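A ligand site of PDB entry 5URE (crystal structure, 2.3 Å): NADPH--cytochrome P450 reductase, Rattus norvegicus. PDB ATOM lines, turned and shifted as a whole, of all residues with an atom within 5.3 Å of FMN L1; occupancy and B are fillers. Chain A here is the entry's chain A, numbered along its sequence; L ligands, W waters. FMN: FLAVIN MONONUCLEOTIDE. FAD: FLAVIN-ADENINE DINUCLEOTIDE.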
ATOM      1  N   GLY A  29     -28.310  27.683 -24.322  1.00  0.00           N
ATOM      2  CA  GLY A  29     -28.429  26.288 -23.967  1.00  0.00           C
ATOM      3  C   GLY A  29     -27.029  26.010 -23.431  1.00  0.00           C
ATOM      4  O   GLY A  29     -26.085  25.833 -24.185  1.00  0.00           O
ATOM      5  N   SER A  30     -26.893  26.059 -22.102  1.00  0.00           N
ATOM      6  CA  SER A  30     -25.602  25.861 -21.469  1.00  0.00           C
ATOM      7  C   SER A  30     -25.629  24.891 -20.295  1.00  0.00           C
ATOM      8  O   SER A  30     -26.536  24.975 -19.463  1.00  0.00           O
ATOM      9  CB  SER A  30     -25.074  27.185 -21.011  1.00  0.00           C
ATOM     10  OG  SER A  30     -23.816  27.079 -20.393  1.00  0.00           O
ATOM     11  N   GLN A  31     -24.602  24.039 -20.154  1.00  0.00           N
ATOM     12  CA  GLN A  31     -24.520  23.097 -19.038  1.00  0.00           C
ATOM     13  C   GLN A  31     -23.550  23.683 -18.049  1.00  0.00           C
ATOM     14  O   GLN A  31     -23.773  23.636 -16.845  1.00  0.00           O
ATOM     15  CB  GLN A  31     -24.037  21.725 -19.517  1.00  0.00           C
ATOM     16  CG  GLN A  31     -24.172  20.592 -18.472  1.00  0.00           C
ATOM     17  CD  GLN A  31     -25.603  20.349 -18.056  1.00  0.00           C
ATOM     18  OE1 GLN A  31     -26.529  20.374 -18.875  1.00  0.00           O
ATOM     19  NE2 GLN A  31     -25.807  20.079 -16.760  1.00  0.00           N
ATOM     20  N   THR A  32     -22.464  24.258 -18.552  1.00  0.00           N
ATOM     21  CA  THR A  32     -21.474  24.847 -17.665  1.00  0.00           C
ATOM     22  C   THR A  32     -21.175  26.339 -17.832  1.00  0.00           C
ATOM     23  O   THR A  32     -20.058  26.792 -17.616  1.00  0.00           O
ATOM     24  CB  THR A  32     -20.158  24.017 -17.691  1.00  0.00           C
ATOM     25  OG1 THR A  32     -19.744  23.804 -19.051  1.00  0.00           O
ATOM     26  CG2 THR A  32     -20.373  22.668 -17.027  1.00  0.00           C
ATOM     27  N   GLY A  33     -22.191  27.111 -18.219  1.00  0.00           N
ATOM     28  CA  GLY A  33     -22.043  28.557 -18.336  1.00  0.00           C
ATOM     29  C   GLY A  33     -21.389  29.239 -19.526  1.00  0.00           C
ATOM     30  O   GLY A  33     -21.427  30.467 -19.611  1.00  0.00           O
ATOM     31  N   THR A  34     -20.801  28.485 -20.442  1.00  0.00           N
ATOM     32  CA  THR A  34     -20.152  29.124 -21.582  1.00  0.00           C
ATOM     33  C   THR A  34     -21.162  29.737 -22.557  1.00  0.00           C
ATOM     34  O   THR A  34     -21.009  30.909 -22.954  1.00  0.00           O
ATOM     35  CB  THR A  34     -19.247  28.127 -22.352  1.00  0.00           C
ATOM     36  OG1 THR A  34     -18.528  27.322 -21.410  1.00  0.00           O
ATOM     37  CG2 THR A  34     -18.243  28.875 -23.199  1.00  0.00           C
ATOM     38  N   ALA A  35     -22.189  28.975 -22.933  1.00  0.00           N
ATOM     39  CA  ALA A  35     -23.194  29.486 -23.858  1.00  0.00           C
ATOM     40  C   ALA A  35     -23.916  30.655 -23.200  1.00  0.00           C
ATOM     41  O   ALA A  35     -24.335  31.613 -23.865  1.00  0.00           O
ATOM     42  CB  ALA A  35     -24.201  28.378 -24.240  1.00  0.00           C
ATOM     43  N   GLU A  36     -24.057  30.576 -21.885  1.00  0.00           N
ATOM     44  CA  GLU A  36     -24.724  31.637 -21.147  1.00  0.00           C
ATOM     45  C   GLU A  36     -23.953  32.945 -21.313  1.00  0.00           C
ATOM     46  O   GLU A  36     -24.548  33.978 -21.630  1.00  0.00           O
ATOM     47  CB  GLU A  36     -24.842  31.281 -19.652  1.00  0.00           C
ATOM     48  CG  GLU A  36     -25.614  32.308 -18.837  1.00  0.00           C
ATOM     49  CD  GLU A  36     -25.815  31.883 -17.389  1.00  0.00           C
ATOM     50  OE1 GLU A  36     -25.497  30.724 -17.031  1.00  0.00           O
ATOM     51  OE2 GLU A  36     -26.303  32.723 -16.607  1.00  0.00           O
ATOM     52  N   ALA A  82     -25.049  24.866 -26.609  1.00  0.00           N
ATOM     53  CA  ALA A  82     -23.960  23.919 -26.419  1.00  0.00           C
ATOM     54  C   ALA A  82     -24.559  22.533 -26.492  1.00  0.00           C
ATOM     55  O   ALA A  82     -25.743  22.355 -26.229  1.00  0.00           O
ATOM     56  CB  ALA A  82     -23.297  24.132 -25.067  1.00  0.00           C
ATOM     57  N   THR A  83     -23.745  21.561 -26.854  1.00  0.00           N
ATOM     58  CA  THR A  83     -24.225  20.193 -26.894  1.00  0.00           C
ATOM     59  C   THR A  83     -23.710  19.527 -25.619  1.00  0.00           C
ATOM     60  O   THR A  83     -22.660  19.904 -25.100  1.00  0.00           O
ATOM     61  CB  THR A  83     -23.665  19.448 -28.105  1.00  0.00           C
ATOM     62  OG1 THR A  83     -24.116  20.076 -29.299  1.00  0.00           O
ATOM     63  CG2 THR A  83     -24.135  17.999 -28.089  1.00  0.00           C
ATOM     64  N   TYR A  84     -24.456  18.549 -25.106  1.00  0.00           N
ATOM     65  CA  TYR A  84     -24.027  17.858 -23.895  1.00  0.00           C
ATOM     66  C   TYR A  84     -24.357  16.383 -23.986  1.00  0.00           C
ATOM     67  O   TYR A  84     -25.120  15.961 -24.857  1.00  0.00           O
ATOM     68  CB  TYR A  84     -24.664  18.466 -22.650  1.00  0.00           C
ATOM     69  CG  TYR A  84     -23.944  18.075 -21.369  1.00  0.00           C
ATOM     70  CD1 TYR A  84     -22.607  18.413 -21.179  1.00  0.00           C
ATOM     71  CD2 TYR A  84     -24.593  17.358 -20.366  1.00  0.00           C
ATOM     72  CE1 TYR A  84     -21.924  18.035 -20.026  1.00  0.00           C
ATOM     73  CE2 TYR A  84     -23.923  16.973 -19.201  1.00  0.00           C
ATOM     74  CZ  TYR A  84     -22.586  17.319 -19.051  1.00  0.00           C
ATOM     75  OH  TYR A  84     -21.896  16.963 -17.914  1.00  0.00           O
ATOM     76  N   GLY A  85     -23.796  15.591 -23.068  1.00  0.00           N
ATOM     77  CA  GLY A  85     -24.027  14.166 -23.077  1.00  0.00           C
ATOM     78  C   GLY A  85     -23.504  13.578 -24.375  1.00  0.00           C
ATOM     79  O   GLY A  85     -22.378  13.864 -24.783  1.00  0.00           O
ATOM     80  N   GLU A  86     -24.313  12.761 -25.038  1.00  0.00           N
ATOM     81  CA  GLU A  86     -23.899  12.163 -26.304  1.00  0.00           C
ATOM     82  C   GLU A  86     -24.749  12.768 -27.427  1.00  0.00           C
ATOM     83  O   GLU A  86     -25.751  12.184 -27.844  1.00  0.00           O
ATOM     84  CB  GLU A  86     -24.087  10.643 -26.248  1.00  0.00           C
ATOM     85  CG  GLU A  86     -23.290   9.876 -27.281  1.00  0.00           C
ATOM     86  CD  GLU A  86     -23.503  10.397 -28.698  1.00  0.00           C
ATOM     87  OE1 GLU A  86     -22.886  11.433 -29.042  1.00  0.00           O
ATOM     88  OE2 GLU A  86     -24.277   9.774 -29.463  1.00  0.00           O
ATOM     89  N   GLY A  87     -24.331  13.929 -27.909  1.00  0.00           N
ATOM     90  CA  GLY A  87     -25.075  14.606 -28.966  1.00  0.00           C
ATOM     91  C   GLY A  87     -26.449  15.009 -28.490  1.00  0.00           C
ATOM     92  O   GLY A  87     -27.414  14.978 -29.255  1.00  0.00           O
ATOM     93  N   ASP A  88     -26.552  15.392 -27.218  1.00  0.00           N
ATOM     94  CA  ASP A  88     -27.816  15.789 -26.607  1.00  0.00           C
ATOM     95  C   ASP A  88     -27.859  17.264 -26.258  1.00  0.00           C
ATOM     96  O   ASP A  88     -26.851  17.971 -26.286  1.00  0.00           O
ATOM     97  CB  ASP A  88     -28.047  15.016 -25.296  1.00  0.00           C
ATOM     98  CG  ASP A  88     -28.154  13.512 -25.480  1.00  0.00           C
ATOM     99  OD1 ASP A  88     -28.943  13.072 -26.351  1.00  0.00           O
ATOM    100  OD2 ASP A  88     -27.467  12.781 -24.743  1.00  0.00           O
ATOM    101  N   THR A  90     -28.415  20.502 -23.706  1.00  0.00           N
ATOM    102  CA  THR A  90     -27.951  20.726 -22.348  1.00  0.00           C
ATOM    103  C   THR A  90     -29.227  20.512 -21.535  1.00  0.00           C
ATOM    104  O   THR A  90     -30.324  20.548 -22.095  1.00  0.00           O
ATOM    105  CB  THR A  90     -27.460  22.174 -22.152  1.00  0.00           C
ATOM    106  OG1 THR A  90     -28.452  23.095 -22.624  1.00  0.00           O
ATOM    107  CG2 THR A  90     -26.176  22.416 -22.936  1.00  0.00           C
ATOM    108  N   LEU A 117     -22.051  25.498 -29.642  1.00  0.00           N
ATOM    109  CA  LEU A 117     -20.858  25.234 -28.848  1.00  0.00           C
ATOM    110  C   LEU A 117     -20.705  23.729 -28.778  1.00  0.00           C
ATOM    111  O   LEU A 117     -21.600  23.022 -28.288  1.00  0.00           O
ATOM    112  CB  LEU A 117     -21.007  25.765 -27.416  1.00  0.00           C
ATOM    113  CG  LEU A 117     -20.869  27.255 -27.147  1.00  0.00           C
ATOM    114  CD1 LEU A 117     -22.119  27.978 -27.682  1.00  0.00           C
ATOM    115  CD2 LEU A 117     -20.699  27.487 -25.622  1.00  0.00           C
ATOM    116  N   GLY A 118     -19.580  23.240 -29.270  1.00  0.00           N
ATOM    117  CA  GLY A 118     -19.334  21.814 -29.258  1.00  0.00           C
ATOM    118  C   GLY A 118     -17.847  21.500 -29.123  1.00  0.00           C
ATOM    119  O   GLY A 118     -17.048  22.359 -28.736  1.00  0.00           O
ATOM    120  N   ASN A 119     -17.489  20.274 -29.446  1.00  0.00           N
ATOM    121  CA  ASN A 119     -16.108  19.820 -29.357  1.00  0.00           C
ATOM    122  C   ASN A 119     -15.920  18.749 -30.411  1.00  0.00           C
ATOM    123  O   ASN A 119     -16.558  17.699 -30.338  1.00  0.00           O
ATOM    124  CB  ASN A 119     -15.849  19.267 -27.962  1.00  0.00           C
ATOM    125  CG  ASN A 119     -14.403  18.883 -27.755  1.00  0.00           C
ATOM    126  OD1 ASN A 119     -13.812  18.189 -28.586  1.00  0.00           O
ATOM    127  ND2 ASN A 119     -13.818  19.338 -26.647  1.00  0.00           N
ATOM    128  N   LYS A 120     -15.057  19.003 -31.387  1.00  0.00           N
ATOM    129  CA  LYS A 120     -14.829  18.045 -32.465  1.00  0.00           C
ATOM    130  C   LYS A 120     -14.372  16.645 -32.070  1.00  0.00           C
ATOM    131  O   LYS A 120     -14.432  15.737 -32.891  1.00  0.00           O
ATOM    132  CB  LYS A 120     -13.830  18.596 -33.477  1.00  0.00           C
ATOM    133  CG  LYS A 120     -14.351  19.720 -34.353  1.00  0.00           C
ATOM    134  CD  LYS A 120     -13.506  19.811 -35.630  1.00  0.00           C
ATOM    135  CE  LYS A 120     -13.931  20.943 -36.537  1.00  0.00           C
ATOM    136  NZ  LYS A 120     -13.521  22.249 -35.971  1.00  0.00           N
ATOM    137  N   TYR A 122     -15.799  14.813 -29.835  1.00  0.00           N
ATOM    138  CA  TYR A 122     -16.979  14.030 -29.480  1.00  0.00           C
ATOM    139  C   TYR A 122     -17.703  13.457 -30.683  1.00  0.00           C
ATOM    140  O   TYR A 122     -17.729  14.055 -31.758  1.00  0.00           O
ATOM    141  CB  TYR A 122     -17.950  14.861 -28.633  1.00  0.00           C
ATOM    142  CG  TYR A 122     -17.471  15.026 -27.213  1.00  0.00           C
ATOM    143  CD1 TYR A 122     -16.345  15.805 -26.929  1.00  0.00           C
ATOM    144  CD2 TYR A 122     -18.117  14.386 -26.150  1.00  0.00           C
ATOM    145  CE1 TYR A 122     -15.877  15.932 -25.616  1.00  0.00           C
ATOM    146  CE2 TYR A 122     -17.647  14.500 -24.842  1.00  0.00           C
ATOM    147  CZ  TYR A 122     -16.518  15.280 -24.580  1.00  0.00           C
ATOM    148  OH  TYR A 122     -16.024  15.393 -23.300  1.00  0.00           O
ATOM    149  N   HIS A 124     -20.830  13.135 -31.856  1.00  0.00           N
ATOM    150  CA  HIS A 124     -21.712  14.011 -32.639  1.00  0.00           C
ATOM    151  C   HIS A 124     -21.400  15.504 -32.419  1.00  0.00           C
ATOM    152  O   HIS A 124     -21.989  16.150 -31.540  1.00  0.00           O
ATOM    153  CB  HIS A 124     -23.176  13.729 -32.294  1.00  0.00           C
ATOM    154  CG  HIS A 124     -23.625  12.358 -32.678  1.00  0.00           C
ATOM    155  ND1 HIS A 124     -23.574  11.290 -31.805  1.00  0.00           N
ATOM    156  CD2 HIS A 124     -24.117  11.866 -33.841  1.00  0.00           C
ATOM    157  CE1 HIS A 124     -24.013  10.207 -32.427  1.00  0.00           C
ATOM    158  NE2 HIS A 124     -24.349  10.535 -33.655  1.00  0.00           N
ATOM    159  N   PHE A 125     -20.505  16.048 -33.225  1.00  0.00           N
ATOM    160  CA  PHE A 125     -20.089  17.440 -33.107  1.00  0.00           C
ATOM    161  C   PHE A 125     -21.183  18.491 -33.293  1.00  0.00           C
ATOM    162  O   PHE A 125     -21.789  18.580 -34.359  1.00  0.00           O
ATOM    163  CB  PHE A 125     -18.953  17.694 -34.113  1.00  0.00           C
ATOM    164  CG  PHE A 125     -18.440  19.109 -34.128  1.00  0.00           C
ATOM    165  CD1 PHE A 125     -18.049  19.728 -32.952  1.00  0.00           C
ATOM    166  CD2 PHE A 125     -18.345  19.814 -35.324  1.00  0.00           C
ATOM    167  CE1 PHE A 125     -17.550  21.026 -32.962  1.00  0.00           C
ATOM    168  CE2 PHE A 125     -17.840  21.110 -35.347  1.00  0.00           C
ATOM    169  CZ  PHE A 125     -17.453  21.717 -34.163  1.00  0.00           C
ATOM    170  N   ASN A 126     -21.415  19.293 -32.247  1.00  0.00           N
ATOM    171  CA  ASN A 126     -22.419  20.361 -32.264  1.00  0.00           C
ATOM    172  C   ASN A 126     -23.810  19.923 -32.672  1.00  0.00           C
ATOM    173  O   ASN A 126     -24.550  20.666 -33.317  1.00  0.00           O
ATOM    174  CB  ASN A 126     -21.983  21.499 -33.203  1.00  0.00           C
ATOM    175  CG  ASN A 126     -21.328  22.663 -32.461  1.00  0.00           C
ATOM    176  OD1 ASN A 126     -20.159  22.977 -32.706  1.00  0.00           O
ATOM    177  ND2 ASN A 126     -22.073  23.300 -31.571  1.00  0.00           N
ATOM    178  N   ALA A 127     -24.172  18.705 -32.265  1.00  0.00           N
ATOM    179  CA  ALA A 127     -25.481  18.155 -32.611  1.00  0.00           C
ATOM    180  C   ALA A 127     -26.634  19.103 -32.300  1.00  0.00           C
ATOM    181  O   ALA A 127     -27.513  19.287 -33.140  1.00  0.00           O
ATOM    182  CB  ALA A 127     -25.697  16.822 -31.888  1.00  0.00           C
ATOM    183  N   ASP A 152     -14.639  23.578 -28.972  1.00  0.00           N
ATOM    184  CA  ASP A 152     -13.922  23.688 -27.712  1.00  0.00           C
ATOM    185  C   ASP A 152     -12.606  22.946 -27.729  1.00  0.00           C
ATOM    186  O   ASP A 152     -11.807  23.064 -26.809  1.00  0.00           O
ATOM    187  CB  ASP A 152     -14.807  23.192 -26.566  1.00  0.00           C
ATOM    188  CG  ASP A 152     -14.436  23.823 -25.229  1.00  0.00           C
ATOM    189  OD1 ASP A 152     -13.637  24.786 -25.218  1.00  0.00           O
ATOM    190  OD2 ASP A 152     -14.956  23.383 -24.191  1.00  0.00           O
ATOM    191  N   LEU A 156     -12.612  27.848 -28.591  1.00  0.00           N
ATOM    192  CA  LEU A 156     -13.997  28.258 -28.706  1.00  0.00           C
ATOM    193  C   LEU A 156     -14.166  29.772 -28.682  1.00  0.00           C
ATOM    194  O   LEU A 156     -14.960  30.322 -29.436  1.00  0.00           O
ATOM    195  CB  LEU A 156     -14.805  27.604 -27.578  1.00  0.00           C
ATOM    196  CG  LEU A 156     -16.282  27.988 -27.573  1.00  0.00           C
ATOM    197  CD1 LEU A 156     -16.941  27.506 -28.857  1.00  0.00           C
ATOM    198  CD2 LEU A 156     -16.978  27.410 -26.347  1.00  0.00           C
ATOM    199  N   VAL A 620     -17.014  10.149 -21.170  1.00  0.00           N
ATOM    200  CA  VAL A 620     -15.724  10.754 -21.504  1.00  0.00           C
ATOM    201  C   VAL A 620     -15.678  12.218 -21.114  1.00  0.00           C
ATOM    202  O   VAL A 620     -16.649  12.960 -21.306  1.00  0.00           O
ATOM    203  CB  VAL A 620     -15.415  10.556 -22.997  1.00  0.00           C
ATOM    204  CG1 VAL A 620     -15.139   9.094 -23.287  1.00  0.00           C
ATOM    205  CG2 VAL A 620     -16.591  11.017 -23.825  1.00  0.00           C
ATOM    206  N   SER A 622     -13.811  16.228 -20.722  1.00  0.00           N
ATOM    207  CA  SER A 622     -13.073  17.319 -21.335  1.00  0.00           C
ATOM    208  C   SER A 622     -13.352  18.557 -20.472  1.00  0.00           C
ATOM    209  O   SER A 622     -14.163  18.459 -19.530  1.00  0.00           O
ATOM    210  CB  SER A 622     -13.599  17.560 -22.755  1.00  0.00           C
ATOM    211  OG  SER A 622     -14.944  18.024 -22.698  1.00  0.00           O
ATOM    212  OXT SER A 622     -12.737  19.622 -20.752  1.00  0.00           O
HETATM  213  N1  FMN L   1     -19.616  18.786 -27.712  1.00  0.00           N
HETATM  214  C2  FMN L   1     -20.153  18.314 -28.858  1.00  0.00           C
HETATM  215  O2  FMN L   1     -20.010  18.909 -29.929  1.00  0.00           O
HETATM  216  N3  FMN L   1     -20.870  17.130 -28.758  1.00  0.00           N
HETATM  217  C4  FMN L   1     -21.095  16.368 -27.618  1.00  0.00           C
HETATM  218  O4  FMN L   1     -21.764  15.358 -27.783  1.00  0.00           O
HETATM  219  C4A FMN L   1     -20.523  16.856 -26.420  1.00  0.00           C
HETATM  220  N5  FMN L   1     -20.720  16.093 -25.243  1.00  0.00           N
HETATM  221  C5A FMN L   1     -20.079  16.615 -24.114  1.00  0.00           C
HETATM  222  C6  FMN L   1     -20.214  15.825 -22.907  1.00  0.00           C
HETATM  223  C7  FMN L   1     -19.595  16.223 -21.697  1.00  0.00           C
HETATM  224  C7M FMN L   1     -19.820  15.274 -20.502  1.00  0.00           C
HETATM  225  C8  FMN L   1     -18.784  17.485 -21.628  1.00  0.00           C
HETATM  226  C8M FMN L   1     -18.120  17.982 -20.524  1.00  0.00           C
HETATM  227  C9  FMN L   1     -18.656  18.246 -22.779  1.00  0.00           C
HETATM  228  C9A FMN L   1     -19.286  17.854 -24.050  1.00  0.00           C
HETATM  229  N10 FMN L   1     -19.166  18.602 -25.312  1.00  0.00           N
HETATM  230  C10 FMN L   1     -19.796  18.087 -26.538  1.00  0.00           C
HETATM  231  C1' FMN L   1     -18.410  19.850 -25.365  1.00  0.00           C
HETATM  232  C2' FMN L   1     -19.257  21.109 -24.972  1.00  0.00           C
HETATM  233  O2' FMN L   1     -20.396  21.231 -25.915  1.00  0.00           O
HETATM  234  C3' FMN L   1     -18.411  22.367 -25.043  1.00  0.00           C
HETATM  235  O3' FMN L   1     -17.341  22.196 -24.090  1.00  0.00           O
HETATM  236  C4' FMN L   1     -19.334  23.587 -24.668  1.00  0.00           C
HETATM  237  O4' FMN L   1     -18.418  24.699 -24.794  1.00  0.00           O
HETATM  238  C5' FMN L   1     -19.810  23.617 -23.227  1.00  0.00           C
HETATM  239  O5' FMN L   1     -20.695  24.769 -23.003  1.00  0.00           O
HETATM  240  P   FMN L   1     -21.395  25.204 -21.663  1.00  0.00           P
HETATM  241  O1P FMN L   1     -20.360  25.629 -20.691  1.00  0.00           O
HETATM  242  O2P FMN L   1     -22.331  23.995 -21.328  1.00  0.00           O
HETATM  243  O3P FMN L   1     -22.158  26.467 -22.263  1.00  0.00           O
HETATM  244  PA  FAD L   2     -10.131  23.314 -12.614  1.00  0.00           P
HETATM  245  O1A FAD L   2      -9.700  24.407 -11.716  1.00  0.00           O
HETATM  246  O2A FAD L   2     -11.544  23.251 -13.038  1.00  0.00           O
HETATM  247  O5B FAD L   2      -9.180  23.327 -13.910  1.00  0.00           O
HETATM  248  C5B FAD L   2      -9.431  22.448 -15.014  1.00  0.00           C
HETATM  249  C4B FAD L   2      -8.590  22.909 -16.205  1.00  0.00           C
HETATM  250  O4B FAD L   2      -7.191  22.961 -15.878  1.00  0.00           O
HETATM  251  C3B FAD L   2      -8.619  21.888 -17.322  1.00  0.00           C
HETATM  252  O3B FAD L   2      -9.867  22.015 -18.032  1.00  0.00           O
HETATM  253  C2B FAD L   2      -7.504  22.463 -18.178  1.00  0.00           C
HETATM  254  O2B FAD L   2      -7.982  23.615 -18.893  1.00  0.00           O
HETATM  255  C1B FAD L   2      -6.482  22.898 -17.135  1.00  0.00           C
HETATM  256  N9A FAD L   2      -5.402  21.899 -16.971  1.00  0.00           N
HETATM  257  C8A FAD L   2      -5.494  20.622 -16.234  1.00  0.00           C
HETATM  258  N7A FAD L   2      -4.092  20.159 -16.337  1.00  0.00           N
HETATM  259  C5A FAD L   2      -3.414  21.014 -17.094  1.00  0.00           C
HETATM  260  C6A FAD L   2      -2.127  20.990 -17.451  1.00  0.00           C
HETATM  261  N6A FAD L   2      -1.376  20.057 -16.863  1.00  0.00           N
HETATM  262  N1A FAD L   2      -1.586  21.910 -18.262  1.00  0.00           N
HETATM  263  C2A FAD L   2      -2.396  22.935 -18.749  1.00  0.00           C
HETATM  264  N3A FAD L   2      -3.740  22.935 -18.366  1.00  0.00           N
HETATM  265  C4A FAD L   2      -4.208  21.984 -17.550  1.00  0.00           C
HETATM  266  N1  FAD L   2     -12.400  13.831 -13.148  1.00  0.00           N
HETATM  267  C2  FAD L   2     -11.941  12.854 -12.260  1.00  0.00           C
HETATM  268  O2  FAD L   2     -10.837  12.984 -11.731  1.00  0.00           O
HETATM  269  N3  FAD L   2     -12.778  11.795 -11.906  1.00  0.00           N
HETATM  270  C4  FAD L   2     -14.072  11.719 -12.416  1.00  0.00           C
HETATM  271  O4  FAD L   2     -14.840  10.851 -12.001  1.00  0.00           O
HETATM  272  C4X FAD L   2     -14.542  12.700 -13.279  1.00  0.00           C
HETATM  273  N5  FAD L   2     -15.704  12.546 -13.922  1.00  0.00           N
HETATM  274  C5X FAD L   2     -16.150  13.513 -14.740  1.00  0.00           C
HETATM  275  C6  FAD L   2     -17.380  13.373 -15.385  1.00  0.00           C
HETATM  276  C7  FAD L   2     -17.838  14.380 -16.230  1.00  0.00           C
HETATM  277  C7M FAD L   2     -19.100  14.267 -16.815  1.00  0.00           C
HETATM  278  C8  FAD L   2     -17.072  15.521 -16.442  1.00  0.00           C
HETATM  279  C8M FAD L   2     -17.528  16.524 -17.278  1.00  0.00           C
HETATM  280  C9  FAD L   2     -15.861  15.670 -15.768  1.00  0.00           C
HETATM  281  C9A FAD L   2     -15.412  14.692 -14.900  1.00  0.00           C
HETATM  282  N10 FAD L   2     -14.238  14.824 -14.256  1.00  0.00           N
HETATM  283  C10 FAD L   2     -13.707  13.752 -13.656  1.00  0.00           C
HETATM  284  C1' FAD L   2     -13.449  16.065 -14.341  1.00  0.00           C
HETATM  285  C2' FAD L   2     -13.894  16.989 -13.204  1.00  0.00           C
HETATM  286  O2' FAD L   2     -15.256  17.358 -13.403  1.00  0.00           O
HETATM  287  C3' FAD L   2     -13.051  18.259 -13.107  1.00  0.00           C
HETATM  288  O3' FAD L   2     -13.044  18.953 -14.362  1.00  0.00           O
HETATM  289  C4' FAD L   2     -11.622  17.938 -12.668  1.00  0.00           C
HETATM  290  O4' FAD L   2     -11.649  17.271 -11.410  1.00  0.00           O
HETATM  291  C5' FAD L   2     -10.833  19.245 -12.546  1.00  0.00           C
HETATM  292  O5' FAD L   2     -11.516  20.128 -11.660  1.00  0.00           O
HETATM  293  P   FAD L   2     -10.708  21.233 -10.811  1.00  0.00           P
HETATM  294  O1P FAD L   2      -9.861  20.526  -9.821  1.00  0.00           O
HETATM  295  O2P FAD L   2     -11.676  22.248 -10.313  1.00  0.00           O
HETATM  296  O3P FAD L   2      -9.748  21.918 -11.909  1.00  0.00           O
HETATM  297  O   HOH W   1     -15.291  20.235 -24.082  1.00  0.00           O
HETATM  298  O   HOH W   2     -22.216  21.389 -22.389  1.00  0.00           O
HETATM  299  O   HOH W   3     -16.535  25.467 -22.651  1.00  0.00           O
HETATM  300  O   HOH W   4     -17.538  21.659 -21.189  1.00  0.00           O
HETATM  301  O   HOH W   5     -21.166  13.335 -29.143  1.00  0.00           O
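The backbone NH (N) of Thr 32 sits at hydrogen-bond distance from an oxygen (O2P) of FMN L1 (2.8 Å). The backbone carbonyl oxygen of Leu 117 is in hydrogen-bond range of an oxygen (O2') of FMN L1 (3.2 Å). An oxygen (O1P) of FMN L1 sits at hydrogen-bond distance from the backbone NH (N) of Thr 34. N3 of FMN L1 sits at hydrogen-bond distance from O of His 124 (3.2 Å). An oxygen (O1P) of FMN L1 sits at hydrogen-bond distance from the backbone NH (N) of Gly 33 (3.4 Å). The backbone NH (N) of Asn 126 sits at hydrogen-bond distance from an oxygen (O2) of FMN L1 (2.7 Å). An oxygen (O1P) of FMN L1 sits at hydrogen-bond distance from the side-chain hydroxyl of Thr 34, at 2.6 Å. The side-chain carboxylate of Asp 152 lies within hydrogen-bond range of an oxygen (O3') of FMN L1 (2.7 Å). The backbone NH of Thr 83 lies within hydrogen-bond range of an oxygen (O2') of FMN L1 (3.5 Å). The backbone carbonyl oxygen of Thr 83 sits at hydrogen-bond distance from an oxygen (O2') of FMN L1 (2.7 Å). OG of Ser 30 is in hydrogen-bond range of O3P of FMN L1, at 2.6 Å. The backbone NH (N) of Gly 87 lies within hydrogen-bond range of an oxygen (O4) of FMN L1, at 2.9 Å. O1P of FMN L1 is in hydrogen-bond range of OG1 of Thr 32 (2.5 Å). The backbone NH (N) of Gln 31 sits at hydrogen-bond distance from an oxygen (O2P) of FMN L1 (2.6 Å). O3P of FMN L1 is in hydrogen-bond range of N of Ala 35, at 2.6 Å. An oxygen (O2) of FMN L1 lies within hydrogen-bond range of the backbone NH (N) of Asn 119 (2.9 Å).
OG1 of Thr 90 is in hydrogen-bond range of N of Ser 30 (3.4 Å). ND2 of Asn 126 sits close to N of Gly 118. O of Gly 118 sits at hydrogen-bond distance from N of Asp 152. ND1 of His 124 sits at hydrogen-bond distance from OE1 of Glu 86. The side-chain carboxylate of Asp 88 is in hydrogen-bond range of the backbone NH of Glu 86. The backbone NH (N) of Thr 83 is in hydrogen-bond range of the backbone carbonyl oxygen (O) of Leu 117. The backbone NH of Thr 34 sits at hydrogen-bond distance from the side-chain hydroxyl of Ser 30 (3.3 Å). N of Ala 82 is in hydrogen-bond range of O of Gly 29, at 2.8 Å.
O of Gly 85 lies close to N5 of FMN L1 (2.8 Å). Residues that only touch FMN L1: Gly 118 (3.1 Å), Tyr 122 (3.2 Å), Ala 82 (3.4 Å), Tyr 84 (3.4 Å), Leu 156 (3.4 Å), Phe 125 (3.5 Å), Ser 622 (3.7 Å) and Glu 86 (3.97 Å). Hydrophobic or aromatic side chains that line FMN L1: Ala 35, Ala 82, Tyr 84, Leu 117, Tyr 122, Phe 125 and Leu 156.
Water W5 lies within hydrogen-bond range of O4 of FMN L1 (2.5 Å), OE1 of Glu 86 (2.6 Å), N of His 124 (2.7 Å) and N of Gly 87 (3.4 Å). Water W2 bridges an oxygen (O2P) of FMN L1 (2.8 Å) and the backbone carbonyl oxygen of Thr 83 (3.1 Å). Water W1 lies within hydrogen-bond range of OG of Ser 622, O3' of FMN L1, ND2 of Asn 119 and OD2 of Asp 152. Water W3 lies within hydrogen-bond range of an oxygen (O4') of FMN L1 (3.0 Å), the side-chain hydroxyl of Thr 34 (3.0 Å) and the side-chain carboxylate of Asp 152 (3.0 Å).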
